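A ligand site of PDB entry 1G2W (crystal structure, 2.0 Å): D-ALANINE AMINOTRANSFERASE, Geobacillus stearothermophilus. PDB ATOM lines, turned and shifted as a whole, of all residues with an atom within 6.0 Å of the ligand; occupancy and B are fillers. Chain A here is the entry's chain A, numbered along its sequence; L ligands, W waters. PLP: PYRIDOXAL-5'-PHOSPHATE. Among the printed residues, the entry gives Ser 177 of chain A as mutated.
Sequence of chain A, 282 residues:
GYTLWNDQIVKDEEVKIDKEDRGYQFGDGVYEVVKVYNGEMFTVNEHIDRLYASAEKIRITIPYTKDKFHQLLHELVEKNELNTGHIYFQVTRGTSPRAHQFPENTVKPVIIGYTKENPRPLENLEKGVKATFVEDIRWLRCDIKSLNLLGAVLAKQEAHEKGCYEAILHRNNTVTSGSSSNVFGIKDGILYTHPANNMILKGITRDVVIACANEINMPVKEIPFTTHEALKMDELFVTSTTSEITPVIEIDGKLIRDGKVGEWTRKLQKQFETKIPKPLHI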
ATOM      1  N   TYR A  31       8.926  30.557  29.389  1.00  0.00           N
ATOM      2  CA  TYR A  31       8.742  31.168  28.084  1.00  0.00           C
ATOM      3  C   TYR A  31       7.268  31.270  27.662  1.00  0.00           C
ATOM      4  O   TYR A  31       6.389  30.668  28.280  1.00  0.00           O
ATOM      5  CB  TYR A  31       9.490  30.360  27.026  1.00  0.00           C
ATOM      6  CG  TYR A  31       8.791  29.068  26.636  1.00  0.00           C
ATOM      7  CD1 TYR A  31       8.811  27.960  27.478  1.00  0.00           C
ATOM      8  CD2 TYR A  31       8.062  28.982  25.443  1.00  0.00           C
ATOM      9  CE1 TYR A  31       8.123  26.787  27.149  1.00  0.00           C
ATOM     10  CE2 TYR A  31       7.382  27.824  25.100  1.00  0.00           C
ATOM     11  CZ  TYR A  31       7.414  26.733  25.963  1.00  0.00           C
ATOM     12  OH  TYR A  31       6.732  25.577  25.633  1.00  0.00           O
ATOM     13  N   GLU A  32       7.041  32.030  26.601  1.00  0.00           N
ATOM     14  CA  GLU A  32       5.719  32.233  26.022  1.00  0.00           C
ATOM     15  C   GLU A  32       5.855  32.378  24.513  1.00  0.00           C
ATOM     16  O   GLU A  32       6.936  32.700  24.002  1.00  0.00           O
ATOM     17  CB  GLU A  32       5.089  33.515  26.569  1.00  0.00           C
ATOM     18  CG  GLU A  32       4.510  33.434  27.970  1.00  0.00           C
ATOM     19  CD  GLU A  32       3.298  32.523  28.040  1.00  0.00           C
ATOM     20  OE1 GLU A  32       2.567  32.412  27.034  1.00  0.00           O
ATOM     21  OE2 GLU A  32       3.068  31.938  29.125  1.00  0.00           O
ATOM     22  N   VAL A  33       4.752  32.101  23.816  1.00  0.00           N
ATOM     23  CA  VAL A  33       4.708  32.280  22.363  1.00  0.00           C
ATOM     24  C   VAL A  33       3.405  33.041  22.101  1.00  0.00           C
ATOM     25  O   VAL A  33       2.337  32.639  22.584  1.00  0.00           O
ATOM     26  CB  VAL A  33       4.675  30.951  21.570  1.00  0.00           C
ATOM     27  CG1 VAL A  33       4.717  31.257  20.067  1.00  0.00           C
ATOM     28  CG2 VAL A  33       5.867  30.083  21.932  1.00  0.00           C
ATOM     29  N   HIS A  47      -0.933  36.372  27.729  1.00  0.00           N
ATOM     30  CA  HIS A  47       0.374  35.714  27.638  1.00  0.00           C
ATOM     31  C   HIS A  47       1.394  36.357  28.578  1.00  0.00           C
ATOM     32  O   HIS A  47       2.207  35.669  29.196  1.00  0.00           O
ATOM     33  CB  HIS A  47       0.869  35.741  26.202  1.00  0.00           C
ATOM     34  CG  HIS A  47       0.260  34.671  25.345  1.00  0.00           C
ATOM     35  ND1 HIS A  47       0.670  33.359  25.390  1.00  0.00           N
ATOM     36  CD2 HIS A  47      -0.758  34.715  24.449  1.00  0.00           C
ATOM     37  CE1 HIS A  47      -0.065  32.636  24.568  1.00  0.00           C
ATOM     38  NE2 HIS A  47      -0.937  33.437  23.992  1.00  0.00           N
ATOM     39  N   ARG A  50       0.630  35.178  32.043  1.00  0.00           N
ATOM     40  CA  ARG A  50       1.113  33.833  32.297  1.00  0.00           C
ATOM     41  C   ARG A  50       2.636  33.754  32.418  1.00  0.00           C
ATOM     42  O   ARG A  50       3.167  32.944  33.172  1.00  0.00           O
ATOM     43  CB  ARG A  50       0.634  32.857  31.223  1.00  0.00           C
ATOM     44  CG  ARG A  50       0.840  31.402  31.619  1.00  0.00           C
ATOM     45  CD  ARG A  50       0.183  30.444  30.625  1.00  0.00           C
ATOM     46  NE  ARG A  50       0.777  30.547  29.296  1.00  0.00           N
ATOM     47  CZ  ARG A  50       0.300  29.934  28.225  1.00  0.00           C
ATOM     48  NH1 ARG A  50      -0.782  29.153  28.326  1.00  0.00           N
ATOM     49  NH2 ARG A  50       0.885  30.099  27.044  1.00  0.00           N
ATOM     50  N   ARG A 138       6.568  13.252  31.528  1.00  0.00           N
ATOM     51  CA  ARG A 138       6.955  14.570  32.009  1.00  0.00           C
ATOM     52  C   ARG A 138       6.952  14.695  33.519  1.00  0.00           C
ATOM     53  O   ARG A 138       6.337  13.883  34.222  1.00  0.00           O
ATOM     54  CB  ARG A 138       6.022  15.626  31.401  1.00  0.00           C
ATOM     55  CG  ARG A 138       6.130  15.736  29.885  1.00  0.00           C
ATOM     56  CD  ARG A 138       5.168  16.764  29.335  1.00  0.00           C
ATOM     57  NE  ARG A 138       3.789  16.392  29.624  1.00  0.00           N
ATOM     58  CZ  ARG A 138       2.725  17.101  29.240  1.00  0.00           C
ATOM     59  NH1 ARG A 138       2.888  18.222  28.539  1.00  0.00           N
ATOM     60  NH2 ARG A 138       1.507  16.671  29.533  1.00  0.00           N
ATOM     61  N   CYS A 142       3.550  20.523  35.175  1.00  0.00           N
ATOM     62  CA  CYS A 142       3.244  20.907  33.813  1.00  0.00           C
ATOM     63  C   CYS A 142       2.444  22.202  33.757  1.00  0.00           C
ATOM     64  O   CYS A 142       2.202  22.733  32.659  1.00  0.00           O
ATOM     65  CB  CYS A 142       2.486  19.787  33.098  1.00  0.00           C
ATOM     66  SG  CYS A 142       3.505  18.336  32.718  1.00  0.00           S
ATOM     67  N   LYS A 145       5.048  26.898  32.409  1.00  0.00           N
ATOM     68  CA  LYS A 145       5.522  26.824  31.029  1.00  0.00           C
ATOM     69  C   LYS A 145       7.045  27.075  31.086  1.00  0.00           C
ATOM     70  O   LYS A 145       7.522  28.174  30.797  1.00  0.00           O
ATOM     71  CB  LYS A 145       4.823  27.885  30.157  1.00  0.00           C
ATOM     72  CG  LYS A 145       4.760  27.504  28.672  1.00  0.00           C
ATOM     73  CD  LYS A 145       4.005  28.535  27.824  1.00  0.00           C
ATOM     74  CE  LYS A 145       3.855  28.051  26.391  1.00  0.00           C
ATOM     75  NZ  LYS A 145       3.254  26.723  26.382  1.00  0.00           N
ATOM     76  N   LEU A 149      11.892  21.030  28.495  1.00  0.00           N
ATOM     77  CA  LEU A 149      11.042  20.448  27.467  1.00  0.00           C
ATOM     78  C   LEU A 149      11.530  19.176  26.813  1.00  0.00           C
ATOM     79  O   LEU A 149      11.087  18.821  25.712  1.00  0.00           O
ATOM     80  CB  LEU A 149      10.810  21.509  26.383  1.00  0.00           C
ATOM     81  CG  LEU A 149      10.043  22.741  26.891  1.00  0.00           C
ATOM     82  CD1 LEU A 149      10.183  23.921  25.920  1.00  0.00           C
ATOM     83  CD2 LEU A 149       8.590  22.341  27.076  1.00  0.00           C
ATOM     84  N   SER A 177      -2.531  15.839  27.687  1.00  0.00           N
ATOM     85  CA  SER A 177      -2.445  16.891  26.677  1.00  0.00           C
ATOM     86  C   SER A 177      -1.493  16.433  25.590  1.00  0.00           C
ATOM     87  O   SER A 177      -0.943  15.337  25.660  1.00  0.00           O
ATOM     88  CB  SER A 177      -1.891  18.184  27.289  1.00  0.00           C
ATOM     89  OG  SER A 177      -0.499  18.059  27.575  1.00  0.00           O
ATOM     90  N   GLY A 178      -1.320  17.264  24.561  1.00  0.00           N
ATOM     91  CA  GLY A 178      -0.388  16.930  23.508  1.00  0.00           C
ATOM     92  C   GLY A 178       0.969  17.391  24.016  1.00  0.00           C
ATOM     93  O   GLY A 178       1.041  17.993  25.093  1.00  0.00           O
ATOM     94  N   SER A 179       2.042  17.126  23.276  1.00  0.00           N
ATOM     95  CA  SER A 179       3.375  17.532  23.716  1.00  0.00           C
ATOM     96  C   SER A 179       3.491  19.053  23.835  1.00  0.00           C
ATOM     97  O   SER A 179       4.253  19.563  24.662  1.00  0.00           O
ATOM     98  CB  SER A 179       4.446  17.005  22.750  1.00  0.00           C
ATOM     99  OG  SER A 179       4.358  17.635  21.481  1.00  0.00           O
ATOM    100  N   SER A 180       2.733  19.775  23.017  1.00  0.00           N
ATOM    101  CA  SER A 180       2.741  21.238  23.053  1.00  0.00           C
ATOM    102  C   SER A 180       1.371  21.824  22.735  1.00  0.00           C
ATOM    103  O   SER A 180       1.258  22.919  22.170  1.00  0.00           O
ATOM    104  CB  SER A 180       3.769  21.790  22.063  1.00  0.00           C
ATOM    105  OG  SER A 180       3.404  21.471  20.737  1.00  0.00           O
ATOM    106  N   SER A 181       0.316  21.090  23.088  1.00  0.00           N
ATOM    107  CA  SER A 181      -1.039  21.559  22.837  1.00  0.00           C
ATOM    108  C   SER A 181      -1.998  20.909  23.828  1.00  0.00           C
ATOM    109  O   SER A 181      -1.646  19.946  24.495  1.00  0.00           O
ATOM    110  CB  SER A 181      -1.470  21.221  21.401  1.00  0.00           C
ATOM    111  OG  SER A 181      -1.438  19.821  21.186  1.00  0.00           O
ATOM    112  N   ASN A 182      -3.210  21.458  23.933  1.00  0.00           N
ATOM    113  CA  ASN A 182      -4.218  20.882  24.822  1.00  0.00           C
ATOM    114  C   ASN A 182      -5.122  20.026  23.947  1.00  0.00           C
ATOM    115  O   ASN A 182      -5.251  20.265  22.745  1.00  0.00           O
ATOM    116  CB  ASN A 182      -4.992  21.983  25.533  1.00  0.00           C
ATOM    117  CG  ASN A 182      -4.146  22.711  26.572  1.00  0.00           C
ATOM    118  OD1 ASN A 182      -3.890  23.912  26.458  1.00  0.00           O
ATOM    119  ND2 ASN A 182      -3.697  21.975  27.597  1.00  0.00           N
ATOM    120  N   LEU A 201      -0.627  22.138  31.018  1.00  0.00           N
ATOM    121  CA  LEU A 201      -0.400  23.569  30.947  1.00  0.00           C
ATOM    122  C   LEU A 201      -1.796  24.118  30.610  1.00  0.00           C
ATOM    123  O   LEU A 201      -2.472  23.600  29.720  1.00  0.00           O
ATOM    124  CB  LEU A 201       0.588  23.879  29.809  1.00  0.00           C
ATOM    125  CG  LEU A 201       1.084  25.323  29.617  1.00  0.00           C
ATOM    126  CD1 LEU A 201      -0.027  26.176  29.069  1.00  0.00           C
ATOM    127  CD2 LEU A 201       1.599  25.871  30.939  1.00  0.00           C
ATOM    128  N   LYS A 202      -2.239  25.128  31.354  1.00  0.00           N
ATOM    129  CA  LYS A 202      -3.552  25.717  31.090  1.00  0.00           C
ATOM    130  C   LYS A 202      -3.419  26.670  29.917  1.00  0.00           C
ATOM    131  O   LYS A 202      -3.163  27.862  30.096  1.00  0.00           O
ATOM    132  CB  LYS A 202      -4.042  26.472  32.322  1.00  0.00           C
ATOM    133  CG  LYS A 202      -5.487  26.881  32.210  1.00  0.00           C
ATOM    134  CD  LYS A 202      -5.901  27.778  33.344  1.00  0.00           C
ATOM    135  CE  LYS A 202      -7.366  28.125  33.232  1.00  0.00           C
ATOM    136  NZ  LYS A 202      -7.705  29.325  34.036  1.00  0.00           N
ATOM    137  N   GLY A 203      -3.601  26.144  28.711  1.00  0.00           N
ATOM    138  CA  GLY A 203      -3.479  26.964  27.515  1.00  0.00           C
ATOM    139  C   GLY A 203      -4.415  28.153  27.408  1.00  0.00           C
ATOM    140  O   GLY A 203      -5.556  28.115  27.881  1.00  0.00           O
ATOM    141  N   ILE A 204      -3.927  29.215  26.785  1.00  0.00           N
ATOM    142  CA  ILE A 204      -4.723  30.407  26.580  1.00  0.00           C
ATOM    143  C   ILE A 204      -5.667  30.118  25.404  1.00  0.00           C
ATOM    144  O   ILE A 204      -6.784  30.629  25.365  1.00  0.00           O
ATOM    145  CB  ILE A 204      -3.818  31.626  26.291  1.00  0.00           C
ATOM    146  CG1 ILE A 204      -3.027  31.975  27.560  1.00  0.00           C
ATOM    147  CG2 ILE A 204      -4.650  32.822  25.831  1.00  0.00           C
ATOM    148  CD1 ILE A 204      -1.921  32.979  27.360  1.00  0.00           C
ATOM    149  N   THR A 205      -5.229  29.291  24.467  1.00  0.00           N
ATOM    150  CA  THR A 205      -6.075  28.931  23.329  1.00  0.00           C
ATOM    151  C   THR A 205      -7.198  28.033  23.872  1.00  0.00           C
ATOM    152  O   THR A 205      -8.361  28.159  23.475  1.00  0.00           O
ATOM    153  CB  THR A 205      -5.302  28.150  22.249  1.00  0.00           C
ATOM    154  OG1 THR A 205      -4.129  28.890  21.873  1.00  0.00           O
ATOM    155  CG2 THR A 205      -6.177  27.955  21.005  1.00  0.00           C
ATOM    156  N   ARG A 206      -6.831  27.150  24.791  1.00  0.00           N
ATOM    157  CA  ARG A 206      -7.768  26.242  25.436  1.00  0.00           C
ATOM    158  C   ARG A 206      -8.867  27.074  26.111  1.00  0.00           C
ATOM    159  O   ARG A 206     -10.055  26.798  25.938  1.00  0.00           O
ATOM    160  CB  ARG A 206      -7.020  25.418  26.488  1.00  0.00           C
ATOM    161  CG  ARG A 206      -7.886  24.709  27.514  1.00  0.00           C
ATOM    162  CD  ARG A 206      -6.984  24.194  28.636  1.00  0.00           C
ATOM    163  NE  ARG A 206      -7.672  23.350  29.601  1.00  0.00           N
ATOM    164  CZ  ARG A 206      -8.494  23.797  30.546  1.00  0.00           C
ATOM    165  NH1 ARG A 206      -8.741  25.083  30.667  1.00  0.00           N
ATOM    166  NH2 ARG A 206      -9.051  22.931  31.386  1.00  0.00           N
ATOM    167  N   THR A 239      -5.314  22.251  20.549  1.00  0.00           N
ATOM    168  CA  THR A 239      -5.212  23.695  20.489  1.00  0.00           C
ATOM    169  C   THR A 239      -3.883  24.187  21.045  1.00  0.00           C
ATOM    170  O   THR A 239      -3.321  23.586  21.952  1.00  0.00           O
ATOM    171  CB  THR A 239      -6.323  24.368  21.328  1.00  0.00           C
ATOM    172  OG1 THR A 239      -6.168  24.010  22.701  1.00  0.00           O
ATOM    173  CG2 THR A 239      -7.712  23.926  20.847  1.00  0.00           C
ATOM    174  N   SER A 240      -3.405  25.289  20.471  1.00  0.00           N
ATOM    175  CA  SER A 240      -2.175  25.934  20.910  1.00  0.00           C
ATOM    176  C   SER A 240      -2.126  27.257  20.161  1.00  0.00           C
ATOM    177  O   SER A 240      -2.838  27.432  19.168  1.00  0.00           O
ATOM    178  CB  SER A 240      -0.943  25.099  20.573  1.00  0.00           C
ATOM    179  OG  SER A 240      -0.560  25.308  19.230  1.00  0.00           O
ATOM    180  N   THR A 241      -1.307  28.175  20.644  1.00  0.00           N
ATOM    181  CA  THR A 241      -1.198  29.492  20.039  1.00  0.00           C
ATOM    182  C   THR A 241      -0.871  29.416  18.544  1.00  0.00           C
ATOM    183  O   THR A 241      -1.399  30.178  17.747  1.00  0.00           O
ATOM    184  CB  THR A 241      -0.133  30.340  20.769  1.00  0.00           C
ATOM    185  OG1 THR A 241      -0.564  30.566  22.109  1.00  0.00           O
ATOM    186  CG2 THR A 241       0.089  31.673  20.065  1.00  0.00           C
ATOM    187  N   THR A 242      -0.014  28.476  18.164  1.00  0.00           N
ATOM    188  CA  THR A 242       0.343  28.348  16.764  1.00  0.00           C
ATOM    189  C   THR A 242      -0.557  27.398  15.972  1.00  0.00           C
ATOM    190  O   THR A 242      -0.693  27.542  14.770  1.00  0.00           O
ATOM    191  CB  THR A 242       1.822  27.910  16.602  1.00  0.00           C
ATOM    192  OG1 THR A 242       2.039  26.690  17.325  1.00  0.00           O
ATOM    193  CG2 THR A 242       2.756  28.994  17.130  1.00  0.00           C
HETATM  194  N1  PLP L   1       0.657  22.483  26.137  1.00  0.00           N
HETATM  195  C2  PLP L   1       1.920  22.694  26.605  1.00  0.00           C
HETATM  196  C2A PLP L   1       2.639  21.511  27.253  1.00  0.00           C
HETATM  197  C3  PLP L   1       2.452  24.009  26.435  1.00  0.00           C
HETATM  198  O3  PLP L   1       3.708  24.176  26.923  1.00  0.00           O
HETATM  199  C4  PLP L   1       1.698  25.050  25.818  1.00  0.00           C
HETATM  200  C4A PLP L   1       2.246  26.398  25.668  1.00  0.00           C
HETATM  201  C5  PLP L   1       0.368  24.671  25.359  1.00  0.00           C
HETATM  202  C6  PLP L   1      -0.129  23.408  25.534  1.00  0.00           C
HETATM  203  C5A PLP L   1      -0.604  25.636  24.650  1.00  0.00           C
HETATM  204  O4P PLP L   1      -0.896  26.803  25.345  1.00  0.00           O
HETATM  205  P   PLP L   1      -1.318  28.045  24.471  1.00  0.00           P
HETATM  206  O1P PLP L   1      -0.326  28.211  23.394  1.00  0.00           O
HETATM  207  O2P PLP L   1      -1.329  29.280  25.388  1.00  0.00           O
HETATM  208  O3P PLP L   1      -2.675  27.783  23.958  1.00  0.00           O
HETATM  209  O   HOH W   1      -4.241  25.568  24.301  1.00  0.00           O
HETATM  210  O   HOH W   2       2.008  30.267  24.154  1.00  0.00           O
HETATM  211  O   HOH W   3       2.353  27.911  22.935  1.00  0.00           O
HETATM  212  O   HOH W   4      -0.497  20.904  28.657  1.00  0.00           O
HETATM  213  O   HOH W   5       5.749  22.976  27.995  1.00  0.00           O
HETATM  214  O   HOH W   6       5.260  19.371  27.288  1.00  0.00           O
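A carbon (C4A) of the ligand is bonded to the side-chain amino group (NZ) of Lys 145 (1.3 Å). N of Thr 241 sits close to O1P of the ligand (2.9 Å). An oxygen (O1P) of the ligand sits close to the side-chain hydroxyl of Thr 241 (2.7 Å). N of Thr 205 lies close to O3P of the ligand, 3.0 Å away. The side-chain hydroxyl (OG1) of Thr 205 lies close to an oxygen (O3P) of the ligand, 2.8 Å away. O2P of the ligand sits close to NH2 of Arg 50, 2.9 Å away. N of Ile 204 sits close to O2P of the ligand (3.0 Å). The backbone NH (N) of Ser 181 sits close to a nitrogen (N1) of the ligand, at 3.4 Å.
The backbone NH (N) of Thr 241 lies within hydrogen-bond range of the side-chain hydroxyl (OG1) of Thr 205 (3.2 Å). OG1 of Thr 241 lies close to NE2 of His 47. O of Ser 240 lies close to OG1 of Thr 205 (3.3 Å). The guanidinium group (NH1) of Arg 50 is in hydrogen-bond range of the backbone carbonyl oxygen (O) of Lys 202, 3.2 Å away. The backbone NH of Gly 203 lies within hydrogen-bond range of the side-chain amide oxygen of Asn 182, 3.2 Å away. The backbone NH (N) of Thr 242 sits close to the side-chain hydroxyl (OG) of Ser 240, at 3.4 Å. The backbone carbonyl oxygen (O) of Leu 201 is in hydrogen-bond range of the side-chain amide nitrogen (ND2) of Asn 182 (2.9 Å). The side-chain carboxylate (OE1) of Glu 32 is in hydrogen-bond range of a ring nitrogen (ND1) of His 47, at 2.7 Å.
Merely in contact with the ligand: Tyr 31 (3.6 Å), His 47 (3.7 Å), Arg 138 (3.5 Å), Ser 179 (3.6 Å), Ser 180 (3.5 Å), Asn 182 (3.9 Å), Leu 201 (3.7 Å), Gly 203 (3.4 Å) and Ser 240 (3.6 Å). Hydrophobic or aromatic side chains that line the ligand: His 47, Leu 201 and Ile 204. Of the 25 residues printed, 15 come within 4 Å of the ligand.
Water W1 lies within hydrogen-bond range of the side-chain amide oxygen of Asn 182 (2.7 Å), the side-chain hydroxyl of Thr 239 (2.9 Å) and the backbone NH of Arg 206 (3.1 Å). Water W4 bridges the backbone NH (N) of Leu 201 (2.7 Å) and the side-chain hydroxyl (OG) of Ser 177 (3.0 Å). Water W2 lies within hydrogen-bond range of the backbone carbonyl oxygen (O) of Val 33 (2.9 Å), the guanidinium group (NH2) of Arg 50 (3.1 Å) and the side-chain hydroxyl (OG1) of Thr 241 (3.3 Å). Water W6 bridges the backbone carbonyl oxygen (O) of Ser 179 (2.8 Å) and the guanidinium group (NH1) of Arg 138 (2.9 Å).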
